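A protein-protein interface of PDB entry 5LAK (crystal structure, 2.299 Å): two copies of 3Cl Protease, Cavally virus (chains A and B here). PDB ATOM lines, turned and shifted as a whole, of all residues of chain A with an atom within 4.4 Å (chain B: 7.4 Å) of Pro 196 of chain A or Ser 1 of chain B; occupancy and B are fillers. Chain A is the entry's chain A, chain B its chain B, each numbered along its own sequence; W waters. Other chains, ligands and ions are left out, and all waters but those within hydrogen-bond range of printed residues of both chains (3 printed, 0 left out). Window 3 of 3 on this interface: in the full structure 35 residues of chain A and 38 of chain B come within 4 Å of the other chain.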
ATOM      1  N   ASP A 145     -25.225  -1.878   1.346  1.00  0.00           N
ATOM      2  CA  ASP A 145     -24.404  -3.076   1.531  1.00  0.00           C
ATOM      3  C   ASP A 145     -23.264  -3.172   0.515  1.00  0.00           C
ATOM      4  O   ASP A 145     -22.761  -4.259   0.240  1.00  0.00           O
ATOM      5  CB  ASP A 145     -25.271  -4.333   1.431  1.00  0.00           C
ATOM      6  CG  ASP A 145     -25.833  -4.557   0.027  1.00  0.00           C
ATOM      7  OD1 ASP A 145     -25.689  -3.670  -0.849  1.00  0.00           O
ATOM      8  OD2 ASP A 145     -26.409  -5.642  -0.206  1.00  0.00           O
ATOM      9  N   SER A 172     -19.159   1.337   9.434  1.00  0.00           N
ATOM     10  CA  SER A 172     -18.701   0.745  10.688  1.00  0.00           C
ATOM     11  C   SER A 172     -18.385  -0.728  10.446  1.00  0.00           C
ATOM     12  O   SER A 172     -18.929  -1.330   9.523  1.00  0.00           O
ATOM     13  CB  SER A 172     -19.750   0.891  11.796  1.00  0.00           C
ATOM     14  OG  SER A 172     -20.882   0.072  11.553  1.00  0.00           O
ATOM     15  N   ASP A 173     -17.505  -1.303  11.263  1.00  0.00           N
ATOM     16  CA  ASP A 173     -17.180  -2.721  11.145  1.00  0.00           C
ATOM     17  C   ASP A 173     -18.332  -3.596  11.599  1.00  0.00           C
ATOM     18  O   ASP A 173     -18.490  -4.718  11.123  1.00  0.00           O
ATOM     19  CB  ASP A 173     -15.932  -3.077  11.957  1.00  0.00           C
ATOM     20  CG  ASP A 173     -14.697  -2.339  11.492  1.00  0.00           C
ATOM     21  OD1 ASP A 173     -14.687  -1.841  10.348  1.00  0.00           O
ATOM     22  OD2 ASP A 173     -13.721  -2.278  12.266  1.00  0.00           O
ATOM     23  N   ASP A 174     -19.129  -3.082  12.528  1.00  0.00           N
ATOM     24  CA  ASP A 174     -20.200  -3.864  13.130  1.00  0.00           C
ATOM     25  C   ASP A 174     -21.324  -2.954  13.618  1.00  0.00           C
ATOM     26  O   ASP A 174     -21.185  -1.735  13.620  1.00  0.00           O
ATOM     27  CB  ASP A 174     -19.631  -4.706  14.281  1.00  0.00           C
ATOM     28  CG  ASP A 174     -20.481  -5.927  14.606  1.00  0.00           C
ATOM     29  OD1 ASP A 174     -21.423  -6.234  13.849  1.00  0.00           O
ATOM     30  OD2 ASP A 174     -20.187  -6.601  15.617  1.00  0.00           O
ATOM     31  N   GLN A 194     -19.972 -10.251  12.691  1.00  0.00           N
ATOM     32  CA  GLN A 194     -19.927  -8.814  12.440  1.00  0.00           C
ATOM     33  C   GLN A 194     -20.841  -8.462  11.262  1.00  0.00           C
ATOM     34  O   GLN A 194     -20.841  -9.147  10.238  1.00  0.00           O
ATOM     35  CB  GLN A 194     -18.506  -8.337  12.151  1.00  0.00           C
ATOM     36  CG  GLN A 194     -17.682  -8.012  13.383  1.00  0.00           C
ATOM     37  CD  GLN A 194     -16.367  -7.351  13.023  1.00  0.00           C
ATOM     38  OE1 GLN A 194     -15.819  -7.586  11.946  1.00  0.00           O
ATOM     39  NE2 GLN A 194     -15.863  -6.501  13.915  1.00  0.00           N
ATOM     40  N   HIS A 195     -21.625  -7.401  11.431  1.00  0.00           N
ATOM     41  CA  HIS A 195     -22.519  -6.884  10.394  1.00  0.00           C
ATOM     42  C   HIS A 195     -22.180  -5.416  10.139  1.00  0.00           C
ATOM     43  O   HIS A 195     -22.744  -4.539  10.789  1.00  0.00           O
ATOM     44  CB  HIS A 195     -23.984  -7.027  10.819  1.00  0.00           C
ATOM     45  CG  HIS A 195     -24.969  -6.580   9.782  1.00  0.00           C
ATOM     46  ND1 HIS A 195     -25.011  -5.289   9.300  1.00  0.00           N
ATOM     47  CD2 HIS A 195     -25.970  -7.245   9.157  1.00  0.00           C
ATOM     48  CE1 HIS A 195     -25.979  -5.184   8.409  1.00  0.00           C
ATOM     49  NE2 HIS A 195     -26.582  -6.355   8.306  1.00  0.00           N
ATOM     50  N   PRO A 196     -21.247  -5.139   9.209  1.00  0.00           N
ATOM     51  CA  PRO A 196     -20.824  -3.750   8.983  1.00  0.00           C
ATOM     52  C   PRO A 196     -21.935  -2.847   8.456  1.00  0.00           C
ATOM     53  O   PRO A 196     -22.914  -3.345   7.902  1.00  0.00           O
ATOM     54  CB  PRO A 196     -19.711  -3.889   7.943  1.00  0.00           C
ATOM     55  CG  PRO A 196     -20.041  -5.131   7.213  1.00  0.00           C
ATOM     56  CD  PRO A 196     -20.599  -6.058   8.256  1.00  0.00           C
ATOM     57  N   SER A 197     -21.777  -1.538   8.648  1.00  0.00           N
ATOM     58  CA  SER A 197     -22.715  -0.555   8.121  1.00  0.00           C
ATOM     59  C   SER A 197     -22.059   0.240   7.007  1.00  0.00           C
ATOM     60  O   SER A 197     -20.854   0.475   7.027  1.00  0.00           O
ATOM     61  CB  SER A 197     -23.200   0.406   9.214  1.00  0.00           C
ATOM     62  OG  SER A 197     -22.159   1.263   9.657  1.00  0.00           O
ATOM     63  N   GLU A 198     -22.868   0.627   6.029  1.00  0.00           N
ATOM     64  CA  GLU A 198     -22.466   1.560   4.986  1.00  0.00           C
ATOM     65  C   GLU A 198     -23.543   2.636   4.928  1.00  0.00           C
ATOM     66  O   GLU A 198     -24.717   2.319   4.740  1.00  0.00           O
ATOM     67  CB  GLU A 198     -22.314   0.864   3.633  1.00  0.00           C
ATOM     68  CG  GLU A 198     -21.360  -0.340   3.597  1.00  0.00           C
ATOM     69  CD  GLU A 198     -19.906   0.041   3.394  1.00  0.00           C
ATOM     70  OE1 GLU A 198     -19.619   1.235   3.176  1.00  0.00           O
ATOM     71  OE2 GLU A 198     -19.044  -0.857   3.429  1.00  0.00           O
ATOM     72  N   LYS A 300     -33.762  -9.223   1.414  1.00  0.00           N
ATOM     73  CA  LYS A 300     -33.479  -8.051   0.592  1.00  0.00           C
ATOM     74  C   LYS A 300     -34.212  -8.097  -0.747  1.00  0.00           C
ATOM     75  O   LYS A 300     -34.934  -7.166  -1.093  1.00  0.00           O
ATOM     76  CB  LYS A 300     -31.980  -7.925   0.307  1.00  0.00           C
ATOM     77  CG  LYS A 300     -31.105  -7.566   1.492  1.00  0.00           C
ATOM     78  CD  LYS A 300     -29.643  -7.658   1.078  1.00  0.00           C
ATOM     79  CE  LYS A 300     -28.699  -7.358   2.222  1.00  0.00           C
ATOM     80  NZ  LYS A 300     -27.284  -7.371   1.757  1.00  0.00           N
ATOM     81  N   SER B   1     -25.469  -7.575   4.245  1.00  0.00           N
ATOM     82  CA  SER B   1     -24.516  -6.488   4.589  1.00  0.00           C
ATOM     83  C   SER B   1     -23.366  -6.446   3.594  1.00  0.00           C
ATOM     84  O   SER B   1     -23.259  -7.300   2.721  1.00  0.00           O
ATOM     85  CB  SER B   1     -23.972  -6.694   6.000  1.00  0.00           C
ATOM     86  OG  SER B   1     -22.921  -7.646   5.986  1.00  0.00           O
ATOM     87  N   ALA B   2     -22.494  -5.457   3.742  1.00  0.00           N
ATOM     88  CA  ALA B   2     -21.333  -5.332   2.869  1.00  0.00           C
ATOM     89  C   ALA B   2     -20.400  -6.540   2.982  1.00  0.00           C
ATOM     90  O   ALA B   2     -19.618  -6.815   2.070  1.00  0.00           O
ATOM     91  CB  ALA B   2     -20.572  -4.046   3.191  1.00  0.00           C
ATOM     92  N   ALA B   3     -20.496  -7.271   4.086  1.00  0.00           N
ATOM     93  CA  ALA B   3     -19.608  -8.403   4.311  1.00  0.00           C
ATOM     94  C   ALA B   3     -19.839  -9.521   3.294  1.00  0.00           C
ATOM     95  O   ALA B   3     -18.931 -10.300   3.006  1.00  0.00           O
ATOM     96  CB  ALA B   3     -19.787  -8.935   5.722  1.00  0.00           C
ATOM     97  N   SER B   4     -21.041  -9.582   2.731  1.00  0.00           N
ATOM     98  CA  SER B   4     -21.405 -10.680   1.842  1.00  0.00           C
ATOM     99  C   SER B   4     -21.647 -10.225   0.402  1.00  0.00           C
ATOM    100  O   SER B   4     -21.926 -11.045  -0.466  1.00  0.00           O
ATOM    101  CB  SER B   4     -22.653 -11.388   2.377  1.00  0.00           C
ATOM    102  N   ASN B   5     -21.511  -8.926   0.145  1.00  0.00           N
ATOM    103  CA  ASN B   5     -21.691  -8.387  -1.203  1.00  0.00           C
ATOM    104  C   ASN B   5     -20.346  -8.238  -1.912  1.00  0.00           C
ATOM    105  O   ASN B   5     -19.515  -7.451  -1.468  1.00  0.00           O
ATOM    106  CB  ASN B   5     -22.402  -7.033  -1.146  1.00  0.00           C
ATOM    107  CG  ASN B   5     -22.729  -6.478  -2.531  1.00  0.00           C
ATOM    108  OD1 ASN B   5     -22.228  -6.958  -3.544  1.00  0.00           O
ATOM    109  ND2 ASN B   5     -23.574  -5.454  -2.569  1.00  0.00           N
ATOM    110  N   PRO B   6     -20.130  -8.982  -3.016  1.00  0.00           N
ATOM    111  CA  PRO B   6     -18.852  -8.900  -3.740  1.00  0.00           C
ATOM    112  C   PRO B   6     -18.496  -7.473  -4.146  1.00  0.00           C
ATOM    113  O   PRO B   6     -17.314  -7.154  -4.251  1.00  0.00           O
ATOM    114  CB  PRO B   6     -19.084  -9.779  -4.977  1.00  0.00           C
ATOM    115  CG  PRO B   6     -20.189 -10.681  -4.612  1.00  0.00           C
ATOM    116  CD  PRO B   6     -21.061  -9.923  -3.666  1.00  0.00           C
ATOM    117  N   SER B   7     -19.507  -6.639  -4.379  1.00  0.00           N
ATOM    118  CA  SER B   7     -19.289  -5.216  -4.621  1.00  0.00           C
ATOM    119  C   SER B   7     -18.318  -4.983  -5.774  1.00  0.00           C
ATOM    120  O   SER B   7     -17.426  -4.138  -5.684  1.00  0.00           O
ATOM    121  CB  SER B   7     -18.760  -4.550  -3.349  1.00  0.00           C
ATOM    122  OG  SER B   7     -19.634  -4.780  -2.257  1.00  0.00           O
ATOM    123  N   THR B 292     -22.539 -15.136   6.138  1.00  0.00           N
ATOM    124  CA  THR B 292     -23.904 -15.126   5.610  1.00  0.00           C
ATOM    125  C   THR B 292     -23.900 -15.502   4.132  1.00  0.00           C
ATOM    126  O   THR B 292     -24.940 -15.487   3.481  1.00  0.00           O
ATOM    127  CB  THR B 292     -24.572 -13.754   5.773  1.00  0.00           C
ATOM    128  OG1 THR B 292     -23.782 -12.756   5.115  1.00  0.00           O
ATOM    129  CG2 THR B 292     -24.721 -13.401   7.248  1.00  0.00           C
HETATM  130  O   HOH W   1     -23.640  -3.228   5.129  1.00  0.00           O
HETATM  131  O   HOH W   2     -26.695  -6.675  -2.415  1.00  0.00           O
HETATM  132  O   HOH W   3     -27.822  -7.044   6.142  1.00  0.00           O
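Of the 10 printed residues of chain A, 5 touch a printed residue of chain B.
Of the 8 printed residues of chain B, 4 touch a printed residue of chain A.
Among the printed residues, no Asp or Glu carboxylate lies within 4 Å of a Lys or Arg side-chain nitrogen of the other chain.
The side-chain amide nitrogen (ND2) of Asn 5 of chain B sits close to the backbone carbonyl oxygen (O) of Asp 145 of chain A (3.2 Å).
NZ of Lys 300 of chain A sits close to N of Ser 1 of chain B.
Among the printed residues, merely in contact across the chains: Asp 145 of chain A with Ala 2 of chain B (3.2 Å), His 195 of chain A with Ser 1 of chain B (3.5 Å), Glu 198 of chain A with Ala 2 of chain B (3.5 Å), Asp 145 of chain A with Ser 1 of chain B (3.6 Å), Pro 196 of chain A with Ser 1 of chain B (3.6 Å) and Pro 196 of chain A with Ala 3 of chain B (3.8 Å).
No position is printed for both chains.
The backbone NH (N) of Ala 3 of chain B sits close to the side-chain hydroxyl (OG) of Ser 1 of chain B (3.1 Å).
The side-chain carboxylate of Asp 174 of chain A is in hydrogen-bond range of the backbone NH of His 195 of chain A (2.7 Å).
The side-chain carboxylate of Asp 145 of chain A lies within salt-bridge range of the side-chain amino group of Lys 300 of chain A, 2.8 Å away.
The backbone carbonyl oxygen (O) of Asn 5 of chain B lies within hydrogen-bond range of the side-chain hydroxyl (OG) of Ser 7 of chain B (2.8 Å).
Pro 196 of chain A touches just these residues of chain B: Ser 1 (3.6 Å) and Ala 3 (3.8 Å).
Printed residues of chain B within 4 Å of Asp 145 of chain A: Ser 1 (3.6 Å), Ala 2 (3.2 Å) and Asn 5 (3.1 Å).
Printed residues of chain A within 4 Å of Ala 2 of chain B: Asp 145 (3.2 Å) and Glu 198 (3.5 Å).
Printed residues of chain A within 4 Å of Ala 3 of chain B: Pro 196 (3.8 Å).
Printed residues of chain B within 4 Å of Glu 198 of chain A: Ala 2 (3.5 Å).
Of the printed residues of chain A, Asn 5 of chain B touches Asp 145.
The nearest residue of chain B that does not touch Pro 196 of chain A is Ala 2 of chain B (4.2 Å).
The nearest printed residue of chain A that does not touch Ser 1 of chain B is Gln 194 of chain A (5.0 Å).
Water W2 bridges the side-chain carboxylate of Asp 145 of chain A (2.5 Å) and the side-chain amide nitrogen of Asn 5 of chain B (3.4 Å).
Water W3 bridges a ring nitrogen (NE2) of His 195 of chain A and the backbone NH of Ser 1 of chain B.
Water W1 bridges N of Ala 2 of chain B and O of Pro 196 of chain A.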
